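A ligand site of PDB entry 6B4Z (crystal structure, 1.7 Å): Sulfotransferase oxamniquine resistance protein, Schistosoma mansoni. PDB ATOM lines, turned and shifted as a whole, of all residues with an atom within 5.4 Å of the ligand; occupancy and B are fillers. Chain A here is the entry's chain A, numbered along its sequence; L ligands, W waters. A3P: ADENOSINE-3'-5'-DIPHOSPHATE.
The backbone NH (N) of Thr 20 lies within hydrogen-bond range of an oxygen (O4P) of the ligand (3.2 Å).
A nitrogen (N6) of the ligand lies within hydrogen-bond range of the backbone carbonyl oxygen of Pro 227 (3.0 Å).
The backbone NH of Gly 21 lies within hydrogen-bond range of an oxygen (O5') of the ligand (3.0 Å).
O6P of the ligand lies within salt-bridge range of NH1 of Arg 19 (2.9 Å).
O5P of the ligand lies within hydrogen-bond range of ND2 of Asn 230 (2.9 Å).
OG of Ser 24 lies within hydrogen-bond range of N7 of the ligand, at 2.8 Å.
The backbone NH of Thr 22 is in hydrogen-bond range of an oxygen (O4P) of the ligand.
N of His 232 lies within hydrogen-bond range of O2P of the ligand.
The guanidinium group of Arg 117 is in salt-bridge range of an oxygen (O1P) of the ligand, at 2.8 Å.
An oxygen (O5P) of the ligand is in hydrogen-bond range of the backbone NH (N) of Lys 23, at 3.0 Å.
OG1 of Thr 22 sits at hydrogen-bond distance from O4P of the ligand.
An oxygen (O4P) of the ligand lies within hydrogen-bond range of the backbone NH (N) of Arg 19, 2.9 Å away.
The side-chain hydroxyl of Ser 125 lies within hydrogen-bond range of an oxygen (O2P) of the ligand, 2.5 Å away.
The guanidinium group (NH2) of Arg 19 lies within hydrogen-bond range of the backbone carbonyl oxygen (O) of Asn 230, 2.9 Å away.
The guanidinium group (NE) of Arg 19 is in hydrogen-bond range of the side-chain hydroxyl (OG) of Ser 125 (2.7 Å).
The backbone NH (N) of Val 229 is in hydrogen-bond range of the side-chain hydroxyl (OG) of Ser 24.
The guanidinium group (NH1) of Arg 117 is in hydrogen-bond range of the backbone carbonyl oxygen (O) of Arg 19 (2.9 Å).
The side-chain hydroxyl (OG) of Ser 24 sits at hydrogen-bond distance from the backbone carbonyl oxygen (O) of Pro 227, at 3.2 Å.
The backbone NH of Lys 23 is in hydrogen-bond range of a ring nitrogen (NE2) of His 39 (3.4 Å).
The side-chain hydroxyl of Thr 20 is in hydrogen-bond range of the backbone carbonyl oxygen of Leu 17, at 2.5 Å.
OG1 of Thr 22 lies within hydrogen-bond range of NE2 of His 39.
Residues that only touch the ligand: Val 229, Ser 231, Leu 205, CAS 228, Tyr 226 and Pro 18.
Hydrophobic or aromatic side chains within 4 Å of the ligand: Leu 205, Tyr 226 and His 232.
Water W7 lies within hydrogen-bond range of O3P of the ligand (2.5 Å) and NE2 of His 232 (3.5 Å).
Water W5 lies within hydrogen-bond range of O1P of the ligand and O of Asp 121.
Water W2 lies within hydrogen-bond range of O5P of the ligand (2.7 Å), N of Ser 24 (2.9 Å), O of Val 229 (3.0 Å) and N of Lys 23 (3.5 Å).
Water W1 lies within hydrogen-bond range of an oxygen (O6P) of the ligand (2.8 Å), the side-chain amide nitrogen (ND2) of Asn 230 (3.1 Å) and the guanidinium group (NH1) of Arg 19 (3.5 Å).
Water W8 lies within hydrogen-bond range of O of Tyr 226 (2.8 Å) and N6 of the ligand (3.3 Å).
Water W9 bridges the backbone NH (N) of Gly 206 (2.8 Å) and a nitrogen (N6) of the ligand (3.5 Å).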
ATOM      1  N   LEU A  17       0.545   7.528  -9.501  1.00  0.00           N
ATOM      2  CA  LEU A  17       1.949   7.501  -9.892  1.00  0.00           C
ATOM      3  C   LEU A  17       2.751   8.550  -9.121  1.00  0.00           C
ATOM      4  O   LEU A  17       2.170   9.495  -8.597  1.00  0.00           O
ATOM      5  CB  LEU A  17       2.078   7.719 -11.398  1.00  0.00           C
ATOM      6  CG  LEU A  17       1.513   6.592 -12.261  1.00  0.00           C
ATOM      7  CD1 LEU A  17       1.439   7.025 -13.722  1.00  0.00           C
ATOM      8  CD2 LEU A  17       2.351   5.325 -12.108  1.00  0.00           C
ATOM      9  N   PRO A  18       4.078   8.377  -9.041  1.00  0.00           N
ATOM     10  CA  PRO A  18       4.882   9.411  -8.399  1.00  0.00           C
ATOM     11  C   PRO A  18       4.715  10.771  -9.076  1.00  0.00           C
ATOM     12  O   PRO A  18       4.421  10.823 -10.269  1.00  0.00           O
ATOM     13  CB  PRO A  18       6.328   8.891  -8.563  1.00  0.00           C
ATOM     14  CG  PRO A  18       6.247   7.890  -9.671  1.00  0.00           C
ATOM     15  CD  PRO A  18       4.903   7.254  -9.524  1.00  0.00           C
ATOM     16  N   ARG A  19       4.877  11.831  -8.290  1.00  0.00           N
ATOM     17  CA  ARG A  19       4.716  13.225  -8.734  1.00  0.00           C
ATOM     18  C   ARG A  19       3.261  13.573  -9.069  1.00  0.00           C
ATOM     19  O   ARG A  19       2.992  14.440  -9.894  1.00  0.00           O
ATOM     20  CB  ARG A  19       5.616  13.523  -9.947  1.00  0.00           C
ATOM     21  CG  ARG A  19       7.091  13.156  -9.757  1.00  0.00           C
ATOM     22  CD  ARG A  19       7.645  13.637  -8.412  1.00  0.00           C
ATOM     23  NE  ARG A  19       7.712  15.096  -8.307  1.00  0.00           N
ATOM     24  CZ  ARG A  19       8.010  15.754  -7.191  1.00  0.00           C
ATOM     25  NH1 ARG A  19       8.264  15.081  -6.074  1.00  0.00           N
ATOM     26  NH2 ARG A  19       8.054  17.084  -7.192  1.00  0.00           N
ATOM     27  N   THR A  20       2.320  12.896  -8.401  1.00  0.00           N
ATOM     28  CA  THR A  20       0.903  13.227  -8.547  1.00  0.00           C
ATOM     29  C   THR A  20       0.287  13.623  -7.203  1.00  0.00           C
ATOM     30  O   THR A  20      -0.923  13.613  -7.034  1.00  0.00           O
ATOM     31  CB  THR A  20       0.087  12.048  -9.132  1.00  0.00           C
ATOM     32  OG1 THR A  20       0.159  10.917  -8.246  1.00  0.00           O
ATOM     33  CG2 THR A  20       0.634  11.657 -10.503  1.00  0.00           C
ATOM     34  N   GLY A  21       1.135  13.999  -6.250  1.00  0.00           N
ATOM     35  CA  GLY A  21       0.682  14.382  -4.926  1.00  0.00           C
ATOM     36  C   GLY A  21       0.630  13.239  -3.930  1.00  0.00           C
ATOM     37  O   GLY A  21      -0.197  13.237  -3.015  1.00  0.00           O
ATOM     38  N   THR A  22       1.522  12.263  -4.090  1.00  0.00           N
ATOM     39  CA  THR A  22       1.521  11.090  -3.220  1.00  0.00           C
ATOM     40  C   THR A  22       1.979  11.405  -1.807  1.00  0.00           C
ATOM     41  O   THR A  22       1.433  10.877  -0.846  1.00  0.00           O
ATOM     42  CB  THR A  22       2.418   9.959  -3.790  1.00  0.00           C
ATOM     43  OG1 THR A  22       3.771  10.406  -3.866  1.00  0.00           O
ATOM     44  CG2 THR A  22       1.933   9.544  -5.173  1.00  0.00           C
ATOM     45  N   LYS A  23       2.988  12.268  -1.671  1.00  0.00           N
ATOM     46  CA  LYS A  23       3.502  12.613  -0.357  1.00  0.00           C
ATOM     47  C   LYS A  23       2.486  13.445   0.425  1.00  0.00           C
ATOM     48  O   LYS A  23       2.325  13.260   1.631  1.00  0.00           O
ATOM     49  CB  LYS A  23       4.839  13.366  -0.462  1.00  0.00           C
ATOM     50  CG  LYS A  23       5.504  13.615   0.885  1.00  0.00           C
ATOM     51  CD  LYS A  23       5.623  12.322   1.682  1.00  0.00           C
ATOM     52  CE  LYS A  23       6.537  12.479   2.894  1.00  0.00           C
ATOM     53  NZ  LYS A  23       6.031  13.409   3.935  1.00  0.00           N
ATOM     54  N   SER A  24       1.822  14.377  -0.254  1.00  0.00           N
ATOM     55  CA  SER A  24       0.755  15.138   0.382  1.00  0.00           C
ATOM     56  C   SER A  24      -0.371  14.215   0.829  1.00  0.00           C
ATOM     57  O   SER A  24      -0.930  14.381   1.917  1.00  0.00           O
ATOM     58  CB  SER A  24       0.218  16.210  -0.568  1.00  0.00           C
ATOM     59  OG  SER A  24       1.141  17.274  -0.700  1.00  0.00           O
ATOM     60  N   HIS A  39       5.057   4.864   1.534  1.00  0.00           N
ATOM     61  CA  HIS A  39       5.493   5.830   0.536  1.00  0.00           C
ATOM     62  C   HIS A  39       6.966   5.519   0.272  1.00  0.00           C
ATOM     63  O   HIS A  39       7.601   4.863   1.099  1.00  0.00           O
ATOM     64  CB  HIS A  39       5.298   7.257   1.039  1.00  0.00           C
ATOM     65  CG  HIS A  39       5.499   8.321  -0.001  1.00  0.00           C
ATOM     66  ND1 HIS A  39       6.745   8.852  -0.298  1.00  0.00           N
ATOM     67  CD2 HIS A  39       4.616   8.970  -0.796  1.00  0.00           C
ATOM     68  CE1 HIS A  39       6.608   9.773  -1.243  1.00  0.00           C
ATOM     69  NE2 HIS A  39       5.330   9.850  -1.567  1.00  0.00           N
ATOM     70  N   ARG A 117      -3.000  14.310 -12.527  1.00  0.00           N
ATOM     71  CA  ARG A 117      -2.748  15.717 -12.838  1.00  0.00           C
ATOM     72  C   ARG A 117      -2.503  15.858 -14.332  1.00  0.00           C
ATOM     73  O   ARG A 117      -2.484  14.865 -15.066  1.00  0.00           O
ATOM     74  CB  ARG A 117      -1.549  16.242 -12.043  1.00  0.00           C
ATOM     75  CG  ARG A 117      -0.228  15.662 -12.518  1.00  0.00           C
ATOM     76  CD  ARG A 117       0.933  16.039 -11.600  1.00  0.00           C
ATOM     77  NE  ARG A 117       1.213  17.477 -11.594  1.00  0.00           N
ATOM     78  CZ  ARG A 117       2.286  18.013 -11.016  1.00  0.00           C
ATOM     79  NH1 ARG A 117       3.181  17.237 -10.428  1.00  0.00           N
ATOM     80  NH2 ARG A 117       2.475  19.326 -11.052  1.00  0.00           N
ATOM     81  N   ASP A 121       2.639  18.600 -16.851  1.00  0.00           N
ATOM     82  CA  ASP A 121       3.106  18.988 -15.530  1.00  0.00           C
ATOM     83  C   ASP A 121       3.743  17.793 -14.827  1.00  0.00           C
ATOM     84  O   ASP A 121       4.786  17.925 -14.174  1.00  0.00           O
ATOM     85  CB  ASP A 121       1.972  19.531 -14.664  1.00  0.00           C
ATOM     86  CG  ASP A 121       1.467  20.890 -15.116  1.00  0.00           C
ATOM     87  OD1 ASP A 121       2.176  21.579 -15.890  1.00  0.00           O
ATOM     88  OD2 ASP A 121       0.372  21.285 -14.683  1.00  0.00           O
ATOM     89  N   SER A 125       7.668  17.430 -13.687  1.00  0.00           N
ATOM     90  CA  SER A 125       7.940  17.137 -12.278  1.00  0.00           C
ATOM     91  C   SER A 125       8.788  15.871 -12.151  1.00  0.00           C
ATOM     92  O   SER A 125       9.712  15.805 -11.341  1.00  0.00           O
ATOM     93  CB  SER A 125       6.619  16.988 -11.505  1.00  0.00           C
ATOM     94  OG  SER A 125       6.835  16.865 -10.110  1.00  0.00           O
ATOM     95  N   VAL A 129      12.853  15.343 -10.537  1.00  0.00           N
ATOM     96  CA  VAL A 129      12.988  14.688  -9.245  1.00  0.00           C
ATOM     97  C   VAL A 129      13.308  13.196  -9.337  1.00  0.00           C
ATOM     98  O   VAL A 129      14.232  12.709  -8.670  1.00  0.00           O
ATOM     99  CB  VAL A 129      11.709  14.858  -8.410  1.00  0.00           C
ATOM    100  CG1 VAL A 129      11.816  14.119  -7.072  1.00  0.00           C
ATOM    101  CG2 VAL A 129      11.404  16.342  -8.183  1.00  0.00           C
ATOM    102  N   LEU A 205      -4.848  16.978  -8.324  1.00  0.00           N
ATOM    103  CA  LEU A 205      -4.124  17.946  -7.504  1.00  0.00           C
ATOM    104  C   LEU A 205      -4.941  19.201  -7.285  1.00  0.00           C
ATOM    105  O   LEU A 205      -5.434  19.805  -8.233  1.00  0.00           O
ATOM    106  CB  LEU A 205      -2.775  18.320  -8.148  1.00  0.00           C
ATOM    107  CG  LEU A 205      -1.605  17.359  -8.024  1.00  0.00           C
ATOM    108  CD1 LEU A 205      -0.385  17.955  -8.716  1.00  0.00           C
ATOM    109  CD2 LEU A 205      -1.311  17.057  -6.561  1.00  0.00           C
ATOM    110  N   GLY A 206      -5.117  19.581  -6.019  1.00  0.00           N
ATOM    111  CA  GLY A 206      -5.905  20.748  -5.679  1.00  0.00           C
ATOM    112  C   GLY A 206      -7.268  20.424  -5.099  1.00  0.00           C
ATOM    113  O   GLY A 206      -7.918  21.294  -4.521  1.00  0.00           O
ATOM    114  N   TYR A 226      -5.164  21.027   3.878  1.00  0.00           N
ATOM    115  CA  TYR A 226      -4.703  19.839   3.157  1.00  0.00           C
ATOM    116  C   TYR A 226      -3.228  20.043   2.789  1.00  0.00           C
ATOM    117  O   TYR A 226      -2.854  21.112   2.319  1.00  0.00           O
ATOM    118  CB  TYR A 226      -5.543  19.589   1.908  1.00  0.00           C
ATOM    119  CG  TYR A 226      -5.201  18.297   1.211  1.00  0.00           C
ATOM    120  CD1 TYR A 226      -5.857  17.110   1.556  1.00  0.00           C
ATOM    121  CD2 TYR A 226      -4.217  18.235   0.234  1.00  0.00           C
ATOM    122  CE1 TYR A 226      -5.544  15.913   0.928  1.00  0.00           C
ATOM    123  CE2 TYR A 226      -3.893  17.046  -0.390  1.00  0.00           C
ATOM    124  CZ  TYR A 226      -4.564  15.887  -0.041  1.00  0.00           C
ATOM    125  OH  TYR A 226      -4.255  14.702  -0.662  1.00  0.00           O
ATOM    126  N   PRO A 227      -2.401  19.014   3.034  1.00  0.00           N
ATOM    127  CA  PRO A 227      -0.950  19.109   2.811  1.00  0.00           C
ATOM    128  C   PRO A 227      -0.567  19.555   1.402  1.00  0.00           C
ATOM    129  O   PRO A 227      -1.190  19.158   0.414  1.00  0.00           O
ATOM    130  CB  PRO A 227      -0.468  17.677   3.075  1.00  0.00           C
ATOM    131  CG  PRO A 227      -1.468  17.138   4.040  1.00  0.00           C
ATOM    132  CD  PRO A 227      -2.791  17.720   3.608  1.00  0.00           C
ATOM    133  N   CAS A 228       0.457  20.401   1.314  1.00  0.00           N
ATOM    134  CA  CAS A 228       1.045  20.790   0.051  1.00  0.00           C
ATOM    135  CB  CAS A 228       0.740  22.237  -0.318  1.00  0.00           C
ATOM    136  C   CAS A 228       2.526  20.661   0.225  1.00  0.00           C
ATOM    137  O   CAS A 228       3.173  21.634   0.657  1.00  0.00           O
ATOM    138  SG  CAS A 228       1.277  22.457  -1.990  1.00  0.00           S
ATOM    139 AS   CAS A 228       3.061  23.757  -1.756  1.00  0.00          AS
ATOM    140  CE1 CAS A 228       4.701  22.730  -2.172  1.00  0.00           C
ATOM    141  CE2 CAS A 228       2.855  25.211  -3.097  1.00  0.00           C
ATOM    142  N   VAL A 229       3.077  19.487  -0.065  1.00  0.00           N
ATOM    143  CA  VAL A 229       4.499  19.241   0.110  1.00  0.00           C
ATOM    144  C   VAL A 229       5.100  18.541  -1.094  1.00  0.00           C
ATOM    145  O   VAL A 229       4.376  18.083  -1.980  1.00  0.00           O
ATOM    146  CB  VAL A 229       4.776  18.381   1.372  1.00  0.00           C
ATOM    147  CG1 VAL A 229       4.392  19.137   2.635  1.00  0.00           C
ATOM    148  CG2 VAL A 229       4.027  17.053   1.286  1.00  0.00           C
ATOM    149  N   ASN A 230       6.429  18.482  -1.122  1.00  0.00           N
ATOM    150  CA  ASN A 230       7.185  17.715  -2.117  1.00  0.00           C
ATOM    151  C   ASN A 230       7.132  18.312  -3.531  1.00  0.00           C
ATOM    152  O   ASN A 230       7.167  17.569  -4.527  1.00  0.00           O
ATOM    153  CB  ASN A 230       6.702  16.253  -2.143  1.00  0.00           C
ATOM    154  CG  ASN A 230       7.769  15.291  -2.622  1.00  0.00           C
ATOM    155  OD1 ASN A 230       8.954  15.618  -2.641  1.00  0.00           O
ATOM    156  ND2 ASN A 230       7.346  14.097  -3.022  1.00  0.00           N
ATOM    157  N   SER A 231       7.081  19.638  -3.638  1.00  0.00           N
ATOM    158  CA  SER A 231       7.211  20.291  -4.939  1.00  0.00           C
ATOM    159  C   SER A 231       8.613  20.067  -5.471  1.00  0.00           C
ATOM    160  O   SER A 231       9.534  19.814  -4.702  1.00  0.00           O
ATOM    161  CB  SER A 231       6.915  21.788  -4.846  1.00  0.00           C
ATOM    162  OG  SER A 231       7.933  22.460  -4.107  1.00  0.00           O
ATOM    163  N   HIS A 232       8.796  20.155  -6.787  1.00  0.00           N
ATOM    164  CA  HIS A 232      10.121  19.909  -7.342  1.00  0.00           C
ATOM    165  C   HIS A 232      11.098  20.997  -6.888  1.00  0.00           C
ATOM    166  O   HIS A 232      12.292  20.748  -6.780  1.00  0.00           O
ATOM    167  CB  HIS A 232      10.080  19.798  -8.878  1.00  0.00           C
ATOM    168  CG  HIS A 232       9.786  21.089  -9.577  1.00  0.00           C
ATOM    169  ND1 HIS A 232      10.733  22.089  -9.733  1.00  0.00           N
ATOM    170  CD2 HIS A 232       8.669  21.538 -10.192  1.00  0.00           C
ATOM    171  CE1 HIS A 232      10.194  23.099 -10.405  1.00  0.00           C
ATOM    172  NE2 HIS A 232       8.944  22.792 -10.692  1.00  0.00           N
ATOM    173  N   HIS A 233      10.581  22.193  -6.607  1.00  0.00           N
ATOM    174  CA  HIS A 233      11.415  23.263  -6.059  1.00  0.00           C
ATOM    175  C   HIS A 233      11.979  22.869  -4.692  1.00  0.00           C
ATOM    176  O   HIS A 233      13.141  23.116  -4.397  1.00  0.00           O
ATOM    177  CB  HIS A 233      10.608  24.567  -5.932  1.00  0.00           C
ATOM    178  CG  HIS A 233      10.279  25.202  -7.248  1.00  0.00           C
ATOM    179  ND1 HIS A 233      11.240  25.646  -8.126  1.00  0.00           N
ATOM    180  CD2 HIS A 233       9.089  25.483  -7.825  1.00  0.00           C
ATOM    181  CE1 HIS A 233      10.653  26.169  -9.191  1.00  0.00           C
ATOM    182  NE2 HIS A 233       9.350  26.090  -9.031  1.00  0.00           N
HETATM  183  P1  A3P L   1       5.554  19.806  -8.789  1.00  0.00           P
HETATM  184  O1P A3P L   1       5.012  20.193 -10.147  1.00  0.00           O
HETATM  185  O2P A3P L   1       6.855  19.026  -8.930  1.00  0.00           O
HETATM  186  O3P A3P L   1       5.785  21.039  -7.952  1.00  0.00           O
HETATM  187  P2  A3P L   1       4.644  13.519  -5.195  1.00  0.00           P
HETATM  188  O4P A3P L   1       3.814  12.324  -5.588  1.00  0.00           O
HETATM  189  O5P A3P L   1       4.577  13.728  -3.705  1.00  0.00           O
HETATM  190  O6P A3P L   1       6.086  13.285  -5.620  1.00  0.00           O
HETATM  191  O5' A3P L   1       4.054  14.786  -5.944  1.00  0.00           O
HETATM  192  C5' A3P L   1       4.572  16.105  -5.728  1.00  0.00           C
HETATM  193  C4' A3P L   1       3.942  17.024  -6.730  1.00  0.00           C
HETATM  194  O4' A3P L   1       2.555  17.291  -6.381  1.00  0.00           O
HETATM  195  C3' A3P L   1       4.617  18.357  -6.772  1.00  0.00           C
HETATM  196  O3' A3P L   1       4.433  18.895  -8.088  1.00  0.00           O
HETATM  197  C2' A3P L   1       3.831  19.134  -5.795  1.00  0.00           C
HETATM  198  O2' A3P L   1       3.972  20.525  -5.999  1.00  0.00           O
HETATM  199  C1' A3P L   1       2.433  18.695  -6.094  1.00  0.00           C
HETATM  200  N9  A3P L   1       1.542  18.872  -5.014  1.00  0.00           N
HETATM  201  C8  A3P L   1       1.581  18.222  -3.843  1.00  0.00           C
HETATM  202  N7  A3P L   1       0.575  18.633  -3.070  1.00  0.00           N
HETATM  203  C5  A3P L   1      -0.148  19.571  -3.758  1.00  0.00           C
HETATM  204  C6  A3P L   1      -1.301  20.365  -3.474  1.00  0.00           C
HETATM  205  N6  A3P L   1      -1.968  20.264  -2.235  1.00  0.00           N
HETATM  206  N1  A3P L   1      -1.753  21.211  -4.416  1.00  0.00           N
HETATM  207  C2  A3P L   1      -1.145  21.324  -5.586  1.00  0.00           C
HETATM  208  N3  A3P L   1      -0.062  20.614  -5.887  1.00  0.00           N
HETATM  209  C4  A3P L   1       0.479  19.728  -5.010  1.00  0.00           C
HETATM  210  O   HOH W   1       8.348  11.816  -4.892  1.00  0.00           O
HETATM  211  O   HOH W   2       2.918  15.572  -2.670  1.00  0.00           O
HETATM  212  O   HOH W   3      -3.366  23.577  -4.023  1.00  0.00           O
HETATM  213  O   HOH W   4      -5.144  20.971  -1.823  1.00  0.00           O
HETATM  214  O   HOH W   5       5.480  20.361 -12.693  1.00  0.00           O
HETATM  215  O   HOH W   6       0.725  21.888  -8.360  1.00  0.00           O
HETATM  216  O   HOH W   7       6.933  23.310  -7.936  1.00  0.00           O
HETATM  217  O   HOH W   8      -3.615  22.235  -0.094  1.00  0.00           O
HETATM  218  O   HOH W   9      -4.861  18.675  -3.384  1.00  0.00           O
HETATM  219  O   HOH W  10       3.229  22.585  -9.386  1.00  0.00           O
